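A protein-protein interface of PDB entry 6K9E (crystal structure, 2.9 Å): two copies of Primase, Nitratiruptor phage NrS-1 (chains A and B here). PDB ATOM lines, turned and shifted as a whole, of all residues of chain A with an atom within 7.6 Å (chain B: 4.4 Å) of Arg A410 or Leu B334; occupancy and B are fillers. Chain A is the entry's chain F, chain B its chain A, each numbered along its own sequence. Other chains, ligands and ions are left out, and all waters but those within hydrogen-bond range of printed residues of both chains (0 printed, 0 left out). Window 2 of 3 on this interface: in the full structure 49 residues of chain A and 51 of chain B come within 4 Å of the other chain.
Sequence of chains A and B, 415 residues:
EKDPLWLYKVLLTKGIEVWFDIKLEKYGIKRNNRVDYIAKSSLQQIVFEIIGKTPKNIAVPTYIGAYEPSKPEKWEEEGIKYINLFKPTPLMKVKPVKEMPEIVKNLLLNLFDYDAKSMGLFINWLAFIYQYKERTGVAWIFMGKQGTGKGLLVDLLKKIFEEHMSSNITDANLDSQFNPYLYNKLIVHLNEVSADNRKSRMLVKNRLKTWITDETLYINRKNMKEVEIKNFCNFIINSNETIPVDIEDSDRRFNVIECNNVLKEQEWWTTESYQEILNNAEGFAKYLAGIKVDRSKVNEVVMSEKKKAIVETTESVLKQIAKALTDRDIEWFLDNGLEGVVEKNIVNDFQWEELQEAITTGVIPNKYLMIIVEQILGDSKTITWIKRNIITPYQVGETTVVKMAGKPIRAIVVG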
ATOM      1  N   VAL A 363      13.639  26.316  27.016  1.00  0.00           N
ATOM      2  CA  VAL A 363      13.617  25.210  26.066  1.00  0.00           C
ATOM      3  C   VAL A 363      12.358  24.411  26.366  1.00  0.00           C
ATOM      4  O   VAL A 363      12.327  23.617  27.310  1.00  0.00           O
ATOM      5  CB  VAL A 363      14.878  24.336  26.176  1.00  0.00           C
ATOM      6  CG1 VAL A 363      14.798  23.174  25.212  1.00  0.00           C
ATOM      7  CG2 VAL A 363      16.123  25.158  25.918  1.00  0.00           C
ATOM      8  N   ILE A 364      11.318  24.609  25.562  1.00  0.00           N
ATOM      9  CA  ILE A 364       9.976  24.137  25.866  1.00  0.00           C
ATOM     10  C   ILE A 364       9.561  23.091  24.833  1.00  0.00           C
ATOM     11  O   ILE A 364       9.437  23.413  23.650  1.00  0.00           O
ATOM     12  CB  ILE A 364       8.958  25.289  25.892  1.00  0.00           C
ATOM     13  CG1 ILE A 364       9.467  26.442  26.754  1.00  0.00           C
ATOM     14  CG2 ILE A 364       7.620  24.802  26.416  1.00  0.00           C
ATOM     15  CD1 ILE A 364       8.871  27.789  26.400  1.00  0.00           C
ATOM     16  N   PRO A 365       9.352  21.838  25.229  1.00  0.00           N
ATOM     17  CA  PRO A 365       8.824  20.842  24.288  1.00  0.00           C
ATOM     18  C   PRO A 365       7.452  21.244  23.770  1.00  0.00           C
ATOM     19  O   PRO A 365       6.651  21.846  24.487  1.00  0.00           O
ATOM     20  CB  PRO A 365       8.727  19.565  25.129  1.00  0.00           C
ATOM     21  CG  PRO A 365       9.566  19.783  26.312  1.00  0.00           C
ATOM     22  CD  PRO A 365       9.799  21.245  26.498  1.00  0.00           C
ATOM     23  N   ASN A 366       7.189  20.907  22.501  1.00  0.00           N
ATOM     24  CA  ASN A 366       5.871  21.155  21.922  1.00  0.00           C
ATOM     25  C   ASN A 366       4.764  20.650  22.837  1.00  0.00           C
ATOM     26  O   ASN A 366       3.714  21.287  22.969  1.00  0.00           O
ATOM     27  CB  ASN A 366       5.754  20.486  20.551  1.00  0.00           C
ATOM     28  CG  ASN A 366       6.437  21.271  19.452  1.00  0.00           C
ATOM     29  OD1 ASN A 366       6.866  22.404  19.653  1.00  0.00           O
ATOM     30  ND2 ASN A 366       6.536  20.668  18.274  1.00  0.00           N
ATOM     31  N   LYS A 367       4.992  19.503  23.479  1.00  0.00           N
ATOM     32  CA  LYS A 367       4.019  18.934  24.404  1.00  0.00           C
ATOM     33  C   LYS A 367       3.630  19.933  25.489  1.00  0.00           C
ATOM     34  O   LYS A 367       2.448  20.090  25.810  1.00  0.00           O
ATOM     35  CB  LYS A 367       4.590  17.655  25.013  1.00  0.00           C
ATOM     36  CG  LYS A 367       3.949  17.236  26.315  1.00  0.00           C
ATOM     37  CD  LYS A 367       4.335  15.814  26.685  1.00  0.00           C
ATOM     38  CE  LYS A 367       3.444  15.275  27.790  1.00  0.00           C
ATOM     39  NZ  LYS A 367       2.352  14.425  27.237  1.00  0.00           N
ATOM     40  N   TYR A 368       4.619  20.606  26.081  1.00  0.00           N
ATOM     41  CA  TYR A 368       4.324  21.559  27.145  1.00  0.00           C
ATOM     42  C   TYR A 368       3.919  22.923  26.604  1.00  0.00           C
ATOM     43  O   TYR A 368       3.195  23.658  27.283  1.00  0.00           O
ATOM     44  CB  TYR A 368       5.531  21.705  28.067  1.00  0.00           C
ATOM     45  CG  TYR A 368       5.857  20.443  28.822  1.00  0.00           C
ATOM     46  CD1 TYR A 368       4.854  19.669  29.386  1.00  0.00           C
ATOM     47  CD2 TYR A 368       7.168  20.017  28.959  1.00  0.00           C
ATOM     48  CE1 TYR A 368       5.151  18.512  30.071  1.00  0.00           C
ATOM     49  CE2 TYR A 368       7.472  18.864  29.640  1.00  0.00           C
ATOM     50  CZ  TYR A 368       6.462  18.115  30.194  1.00  0.00           C
ATOM     51  OH  TYR A 368       6.773  16.964  30.870  1.00  0.00           O
ATOM     52  N   LEU A 369       4.385  23.291  25.409  1.00  0.00           N
ATOM     53  CA  LEU A 369       3.970  24.558  24.812  1.00  0.00           C
ATOM     54  C   LEU A 369       2.459  24.609  24.626  1.00  0.00           C
ATOM     55  O   LEU A 369       1.828  25.644  24.867  1.00  0.00           O
ATOM     56  CB  LEU A 369       4.680  24.771  23.476  1.00  0.00           C
ATOM     57  CG  LEU A 369       5.168  26.177  23.113  1.00  0.00           C
ATOM     58  CD1 LEU A 369       5.337  26.303  21.611  1.00  0.00           C
ATOM     59  CD2 LEU A 369       4.271  27.278  23.649  1.00  0.00           C
ATOM     60  N   ILE A 383       0.140  23.813  17.465  1.00  0.00           N
ATOM     61  CA  ILE A 383       1.496  24.337  17.344  1.00  0.00           C
ATOM     62  C   ILE A 383       1.579  25.327  16.193  1.00  0.00           C
ATOM     63  O   ILE A 383       2.235  26.371  16.297  1.00  0.00           O
ATOM     64  CB  ILE A 383       2.499  23.184  17.179  1.00  0.00           C
ATOM     65  CG1 ILE A 383       2.655  22.432  18.498  1.00  0.00           C
ATOM     66  CG2 ILE A 383       3.835  23.711  16.701  1.00  0.00           C
ATOM     67  CD1 ILE A 383       3.353  23.239  19.570  1.00  0.00           C
ATOM     68  N   LYS A 387       2.950  29.215  16.690  1.00  0.00           N
ATOM     69  CA  LYS A 387       4.049  29.839  15.961  1.00  0.00           C
ATOM     70  C   LYS A 387       3.585  31.050  15.166  1.00  0.00           C
ATOM     71  O   LYS A 387       4.292  32.059  15.102  1.00  0.00           O
ATOM     72  CB  LYS A 387       4.720  28.818  15.045  1.00  0.00           C
ATOM     73  CG  LYS A 387       5.178  27.557  15.756  1.00  0.00           C
ATOM     74  CD  LYS A 387       5.596  26.476  14.771  1.00  0.00           C
ATOM     75  CE  LYS A 387       6.511  27.022  13.685  1.00  0.00           C
ATOM     76  NZ  LYS A 387       7.797  27.531  14.216  1.00  0.00           N
ATOM     77  N   THR A 399      11.829  26.901  16.726  1.00  0.00           N
ATOM     78  CA  THR A 399      11.471  25.517  16.999  1.00  0.00           C
ATOM     79  C   THR A 399      12.416  24.588  16.253  1.00  0.00           C
ATOM     80  O   THR A 399      12.685  24.781  15.064  1.00  0.00           O
ATOM     81  CB  THR A 399      10.025  25.234  16.599  1.00  0.00           C
ATOM     82  OG1 THR A 399       9.950  25.033  15.184  1.00  0.00           O
ATOM     83  CG2 THR A 399       9.133  26.387  16.991  1.00  0.00           C
ATOM     84  N   THR A 400      12.907  23.573  16.953  1.00  0.00           N
ATOM     85  CA  THR A 400      13.992  22.743  16.456  1.00  0.00           C
ATOM     86  C   THR A 400      13.980  21.451  17.256  1.00  0.00           C
ATOM     87  O   THR A 400      13.383  21.375  18.331  1.00  0.00           O
ATOM     88  CB  THR A 400      15.343  23.461  16.562  1.00  0.00           C
ATOM     89  OG1 THR A 400      16.316  22.777  15.762  1.00  0.00           O
ATOM     90  CG2 THR A 400      15.812  23.518  18.005  1.00  0.00           C
ATOM     91  N   VAL A 401      14.637  20.429  16.719  1.00  0.00           N
ATOM     92  CA  VAL A 401      14.727  19.161  17.432  1.00  0.00           C
ATOM     93  C   VAL A 401      15.852  19.245  18.451  1.00  0.00           C
ATOM     94  O   VAL A 401      17.001  19.535  18.104  1.00  0.00           O
ATOM     95  CB  VAL A 401      14.951  17.994  16.465  1.00  0.00           C
ATOM     96  CG1 VAL A 401      14.725  16.678  17.185  1.00  0.00           C
ATOM     97  CG2 VAL A 401      14.039  18.124  15.266  1.00  0.00           C
ATOM     98  N   VAL A 402      15.522  18.970  19.707  1.00  0.00           N
ATOM     99  CA  VAL A 402      16.471  19.009  20.810  1.00  0.00           C
ATOM    100  C   VAL A 402      16.428  17.671  21.533  1.00  0.00           C
ATOM    101  O   VAL A 402      15.368  17.048  21.652  1.00  0.00           O
ATOM    102  CB  VAL A 402      16.179  20.191  21.762  1.00  0.00           C
ATOM    103  CG1 VAL A 402      15.200  19.800  22.849  1.00  0.00           C
ATOM    104  CG2 VAL A 402      17.469  20.678  22.391  1.00  0.00           C
ATOM    105  N   LYS A 403      17.595  17.211  21.976  1.00  0.00           N
ATOM    106  CA  LYS A 403      17.749  15.903  22.602  1.00  0.00           C
ATOM    107  C   LYS A 403      17.749  16.089  24.115  1.00  0.00           C
ATOM    108  O   LYS A 403      18.744  16.543  24.690  1.00  0.00           O
ATOM    109  CB  LYS A 403      19.037  15.224  22.141  1.00  0.00           C
ATOM    110  CG  LYS A 403      18.946  14.510  20.801  1.00  0.00           C
ATOM    111  CD  LYS A 403      20.278  13.855  20.461  1.00  0.00           C
ATOM    112  CE  LYS A 403      20.269  13.225  19.076  1.00  0.00           C
ATOM    113  NZ  LYS A 403      21.652  12.900  18.612  1.00  0.00           N
ATOM    114  N   MET A 404      16.641  15.741  24.759  1.00  0.00           N
ATOM    115  CA  MET A 404      16.578  15.712  26.211  1.00  0.00           C
ATOM    116  C   MET A 404      16.312  14.286  26.664  1.00  0.00           C
ATOM    117  O   MET A 404      15.521  13.566  26.045  1.00  0.00           O
ATOM    118  CB  MET A 404      15.517  16.671  26.751  1.00  0.00           C
ATOM    119  CG  MET A 404      14.191  16.622  26.044  1.00  0.00           C
ATOM    120  SD  MET A 404      13.137  17.945  26.655  1.00  0.00           S
ATOM    121  CE  MET A 404      14.273  19.328  26.580  1.00  0.00           C
ATOM    122  N   LYS A 407      15.780  10.736  23.931  1.00  0.00           N
ATOM    123  CA  LYS A 407      14.926  10.862  22.764  1.00  0.00           C
ATOM    124  C   LYS A 407      15.120  12.212  22.078  1.00  0.00           C
ATOM    125  O   LYS A 407      15.589  13.174  22.693  1.00  0.00           O
ATOM    126  CB  LYS A 407      13.465  10.689  23.166  1.00  0.00           C
ATOM    127  N   PRO A 408      14.781  12.301  20.785  1.00  0.00           N
ATOM    128  CA  PRO A 408      14.763  13.605  20.110  1.00  0.00           C
ATOM    129  C   PRO A 408      13.392  14.271  20.177  1.00  0.00           C
ATOM    130  O   PRO A 408      12.478  13.920  19.422  1.00  0.00           O
ATOM    131  CB  PRO A 408      15.151  13.251  18.672  1.00  0.00           C
ATOM    132  CG  PRO A 408      14.623  11.864  18.488  1.00  0.00           C
ATOM    133  CD  PRO A 408      14.661  11.183  19.834  1.00  0.00           C
ATOM    134  N   ILE A 409      13.238  15.246  21.072  1.00  0.00           N
ATOM    135  CA  ILE A 409      11.956  15.890  21.340  1.00  0.00           C
ATOM    136  C   ILE A 409      11.918  17.231  20.627  1.00  0.00           C
ATOM    137  O   ILE A 409      12.821  18.061  20.791  1.00  0.00           O
ATOM    138  CB  ILE A 409      11.716  16.054  22.852  1.00  0.00           C
ATOM    139  CG1 ILE A 409      11.236  14.728  23.455  1.00  0.00           C
ATOM    140  CG2 ILE A 409      10.721  17.169  23.128  1.00  0.00           C
ATOM    141  CD1 ILE A 409      11.544  14.557  24.943  1.00  0.00           C
ATOM    142  N   ARG A 410      10.877  17.442  19.832  1.00  0.00           N
ATOM    143  CA  ARG A 410      10.688  18.713  19.152  1.00  0.00           C
ATOM    144  C   ARG A 410      10.341  19.793  20.163  1.00  0.00           C
ATOM    145  O   ARG A 410       9.398  19.640  20.945  1.00  0.00           O
ATOM    146  CB  ARG A 410       9.574  18.575  18.133  1.00  0.00           C
ATOM    147  CG  ARG A 410       9.827  17.462  17.179  1.00  0.00           C
ATOM    148  CD  ARG A 410      10.040  18.080  15.843  1.00  0.00           C
ATOM    149  NE  ARG A 410      10.569  17.164  14.850  1.00  0.00           N
ATOM    150  CZ  ARG A 410      11.048  17.564  13.681  1.00  0.00           C
ATOM    151  NH1 ARG A 410      11.525  16.681  12.815  1.00  0.00           N
ATOM    152  NH2 ARG A 410      11.040  18.856  13.389  1.00  0.00           N
ATOM    153  N   ALA A 411      11.087  20.893  20.141  1.00  0.00           N
ATOM    154  CA  ALA A 411      10.892  21.952  21.117  1.00  0.00           C
ATOM    155  C   ALA A 411      11.184  23.289  20.460  1.00  0.00           C
ATOM    156  O   ALA A 411      11.655  23.357  19.322  1.00  0.00           O
ATOM    157  CB  ALA A 411      11.780  21.747  22.346  1.00  0.00           C
ATOM    158  N   ILE A 412      10.895  24.359  21.193  1.00  0.00           N
ATOM    159  CA  ILE A 412      11.227  25.717  20.784  1.00  0.00           C
ATOM    160  C   ILE A 412      12.262  26.257  21.760  1.00  0.00           C
ATOM    161  O   ILE A 412      12.070  26.190  22.979  1.00  0.00           O
ATOM    162  CB  ILE A 412       9.983  26.618  20.738  1.00  0.00           C
ATOM    163  CG1 ILE A 412      10.408  28.071  20.587  1.00  0.00           C
ATOM    164  CG2 ILE A 412       9.122  26.424  21.972  1.00  0.00           C
ATOM    165  CD1 ILE A 412       9.324  29.040  20.886  1.00  0.00           C
ATOM    166  N   ILE B 330       8.367  16.926   4.904  1.00  0.00           N
ATOM    167  CA  ILE B 330       7.917  16.229   6.101  1.00  0.00           C
ATOM    168  C   ILE B 330       8.273  17.016   7.349  1.00  0.00           C
ATOM    169  O   ILE B 330       7.534  16.983   8.337  1.00  0.00           O
ATOM    170  CB  ILE B 330       8.508  14.802   6.137  1.00  0.00           C
ATOM    171  CG1 ILE B 330       7.956  14.027   7.327  1.00  0.00           C
ATOM    172  CG2 ILE B 330      10.031  14.855   6.226  1.00  0.00           C
ATOM    173  CD1 ILE B 330       6.452  13.950   7.330  1.00  0.00           C
ATOM    174  N   GLU B 331       9.366  17.780   7.306  1.00  0.00           N
ATOM    175  CA  GLU B 331       9.852  18.459   8.498  1.00  0.00           C
ATOM    176  C   GLU B 331       9.057  19.734   8.781  1.00  0.00           C
ATOM    177  O   GLU B 331       8.970  20.161   9.942  1.00  0.00           O
ATOM    178  CB  GLU B 331      11.342  18.753   8.354  1.00  0.00           C
ATOM    179  CG  GLU B 331      11.944  19.733   9.381  1.00  0.00           C
ATOM    180  CD  GLU B 331      12.367  19.027  10.665  1.00  0.00           C
ATOM    181  OE1 GLU B 331      12.650  17.812  10.565  1.00  0.00           O
ATOM    182  OE2 GLU B 331      12.382  19.657  11.762  1.00  0.00           O
ATOM    183  N   TRP B 332       8.446  20.346   7.754  1.00  0.00           N
ATOM    184  CA  TRP B 332       7.512  21.435   8.020  1.00  0.00           C
ATOM    185  C   TRP B 332       6.351  20.928   8.857  1.00  0.00           C
ATOM    186  O   TRP B 332       5.918  21.592   9.801  1.00  0.00           O
ATOM    187  CB  TRP B 332       6.996  22.048   6.715  1.00  0.00           C
ATOM    188  CG  TRP B 332       6.057  23.198   6.973  1.00  0.00           C
ATOM    189  CD1 TRP B 332       6.381  24.516   7.020  1.00  0.00           C
ATOM    190  CD2 TRP B 332       4.648  23.126   7.235  1.00  0.00           C
ATOM    191  NE1 TRP B 332       5.271  25.273   7.289  1.00  0.00           N
ATOM    192  CE2 TRP B 332       4.193  24.443   7.427  1.00  0.00           C
ATOM    193  CE3 TRP B 332       3.728  22.078   7.324  1.00  0.00           C
ATOM    194  CZ2 TRP B 332       2.862  24.740   7.700  1.00  0.00           C
ATOM    195  CZ3 TRP B 332       2.409  22.375   7.599  1.00  0.00           C
ATOM    196  CH2 TRP B 332       1.988  23.694   7.782  1.00  0.00           C
ATOM    197  N   PHE B 333       5.803  19.767   8.492  1.00  0.00           N
ATOM    198  CA  PHE B 333       4.678  19.219   9.235  1.00  0.00           C
ATOM    199  C   PHE B 333       5.073  18.886  10.667  1.00  0.00           C
ATOM    200  O   PHE B 333       4.297  19.117  11.600  1.00  0.00           O
ATOM    201  CB  PHE B 333       4.130  17.995   8.510  1.00  0.00           C
ATOM    202  CG  PHE B 333       3.333  18.333   7.284  1.00  0.00           C
ATOM    203  CD1 PHE B 333       2.068  18.874   7.401  1.00  0.00           C
ATOM    204  CD2 PHE B 333       3.843  18.108   6.020  1.00  0.00           C
ATOM    205  CE1 PHE B 333       1.333  19.188   6.290  1.00  0.00           C
ATOM    206  CE2 PHE B 333       3.104  18.417   4.900  1.00  0.00           C
ATOM    207  CZ  PHE B 333       1.847  18.957   5.039  1.00  0.00           C
ATOM    208  N   LEU B 334       6.281  18.355  10.866  1.00  0.00           N
ATOM    209  CA  LEU B 334       6.693  18.009  12.219  1.00  0.00           C
ATOM    210  C   LEU B 334       7.086  19.237  13.025  1.00  0.00           C
ATOM    211  O   LEU B 334       6.906  19.249  14.245  1.00  0.00           O
ATOM    212  CB  LEU B 334       7.849  17.012  12.181  1.00  0.00           C
ATOM    213  CG  LEU B 334       7.684  15.795  11.271  1.00  0.00           C
ATOM    214  CD1 LEU B 334       9.021  15.165  10.972  1.00  0.00           C
ATOM    215  CD2 LEU B 334       6.761  14.777  11.906  1.00  0.00           C
ATOM    216  N   ASP B 335       7.608  20.280  12.374  1.00  0.00           N
ATOM    217  CA  ASP B 335       7.771  21.557  13.063  1.00  0.00           C
ATOM    218  C   ASP B 335       6.434  22.110  13.524  1.00  0.00           C
ATOM    219  O   ASP B 335       6.368  22.814  14.537  1.00  0.00           O
ATOM    220  CB  ASP B 335       8.479  22.575  12.169  1.00  0.00           C
ATOM    221  CG  ASP B 335       9.977  22.592  12.377  1.00  0.00           C
ATOM    222  OD1 ASP B 335      10.468  21.828  13.234  1.00  0.00           O
ATOM    223  OD2 ASP B 335      10.664  23.388  11.703  1.00  0.00           O
ATOM    224  N   ASN B 336       5.364  21.815  12.791  1.00  0.00           N
ATOM    225  CA  ASN B 336       4.036  22.282  13.146  1.00  0.00           C
ATOM    226  C   ASN B 336       3.237  21.229  13.897  1.00  0.00           C
ATOM    227  O   ASN B 336       2.004  21.279  13.896  1.00  0.00           O
ATOM    228  CB  ASN B 336       3.290  22.735  11.893  1.00  0.00           C
ATOM    229  CG  ASN B 336       3.912  23.961  11.259  1.00  0.00           C
ATOM    230  OD1 ASN B 336       3.434  25.079  11.433  1.00  0.00           O
ATOM    231  ND2 ASN B 336       4.983  23.754  10.509  1.00  0.00           N
ATOM    232  N   GLY B 337       3.911  20.267  14.522  1.00  0.00           N
ATOM    233  CA  GLY B 337       3.253  19.406  15.484  1.00  0.00           C
ATOM    234  C   GLY B 337       2.466  18.256  14.907  1.00  0.00           C
ATOM    235  O   GLY B 337       1.477  17.832  15.511  1.00  0.00           O
ATOM    236  N   LEU B 338       2.861  17.741  13.744  1.00  0.00           N
ATOM    237  CA  LEU B 338       2.089  16.659  13.146  1.00  0.00           C
ATOM    238  C   LEU B 338       2.164  15.378  13.966  1.00  0.00           C
ATOM    239  O   LEU B 338       1.216  14.592  13.959  1.00  0.00           O
ATOM    240  CB  LEU B 338       2.559  16.408  11.711  1.00  0.00           C
ATOM    241  CG  LEU B 338       2.003  15.163  11.021  1.00  0.00           C
ATOM    242  CD1 LEU B 338       0.500  15.268  10.878  1.00  0.00           C
ATOM    243  CD2 LEU B 338       2.640  14.943   9.670  1.00  0.00           C
ATOM    244  N   TRP B 352       1.411   5.588  11.281  1.00  0.00           N
ATOM    245  CA  TRP B 352       2.169   6.824  11.436  1.00  0.00           C
ATOM    246  C   TRP B 352       3.363   6.874  10.503  1.00  0.00           C
ATOM    247  O   TRP B 352       3.828   7.966  10.167  1.00  0.00           O
ATOM    248  CB  TRP B 352       2.643   6.994  12.876  1.00  0.00           C
ATOM    249  CG  TRP B 352       3.664   8.087  13.072  1.00  0.00           C
ATOM    250  CD1 TRP B 352       4.902   7.957  13.627  1.00  0.00           C
ATOM    251  CD2 TRP B 352       3.539   9.466  12.700  1.00  0.00           C
ATOM    252  NE1 TRP B 352       5.549   9.165  13.636  1.00  0.00           N
ATOM    253  CE2 TRP B 352       4.733  10.110  13.072  1.00  0.00           C
ATOM    254  CE3 TRP B 352       2.531  10.220  12.091  1.00  0.00           C
ATOM    255  CZ2 TRP B 352       4.951  11.467  12.853  1.00  0.00           C
ATOM    256  CZ3 TRP B 352       2.748  11.568  11.876  1.00  0.00           C
ATOM    257  CH2 TRP B 352       3.946  12.177  12.256  1.00  0.00           C
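The guanidinium group (NH1) of Arg A410 is in salt-bridge range of the side-chain carboxylate (OE1) of Glu B331 (2.8 Å). NH2 of Arg A410 is in salt-bridge range of OD1 of Asp B335 (3.0 Å).
The backbone carbonyl oxygen (O) of Trp B332 lies within hydrogen-bond range of the side-chain amide nitrogen (ND2) of Asn B336, at 2.5 Å. O of Arg A410 is in hydrogen-bond range of N of Asn A366, 3.0 Å away. The side-chain amino group of Lys A387 lies close to the side-chain hydroxyl of Thr A399 (3.4 Å).
CG2 of Ile A383 touches O of Asp B335 (3.5 Å). CG2 of Ile A383 touches C of Asn B336, 3.8 Å away. CD of Lys A387 touches O of Asp B335 (3.7 Å). OG1 of Thr A399 touches CG of Asp B335, 3.7 Å away. NH1 of Arg A410 touches CD1 of Leu B334, at 3.5 Å.
Of the printed residues of chain B, Arg A410 touches Glu B331 (2.3 Å), Leu B334 (3.5 Å) and Asp B335 (3.0 Å). Printed residues of chain A within 4 Å of Leu B334: Arg A410 (3.5 Å). Of the printed residues of chain A, Asp B335 touches Ile A383 (3.5 Å), Lys A387 (3.7 Å), Thr A399 (3.7 Å) and Arg A410 (3.0 Å). Of the printed residues of chain B, Thr A399 touches Asp B335. Of the printed residues of chain A, Asn B336 touches Ile A383 (3.8 Å). The nearest printed residue of chain B that does not touch Arg A410 is Ile B330 (6.0 Å). The nearest residue of chain A that does not touch Leu B334 is Asn A366 (4.3 Å).
Of the 10 printed residues of chain B, 4 touch a printed residue of chain A. Hydrophobic or aromatic side chains of chain B that line the printed part of chain A: Leu B334. Along chain B the printed residues that touch a printed residue of chain A span positions 331 to 336. Among the printed residues, 7 pairs touch across the chains. Among the printed residues, Asp or Glu carboxylates within 4 Å of a Lys or Arg side-chain nitrogen of the other chain: Arg A410 with Glu B331 (2.3 Å) and Arg A410 with Asp B335 (3.0 Å).
No position is printed for both chains. Of the 7 pairs that touch across the chains among the printed residues, none has its exchanged pair printed and touching as well.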
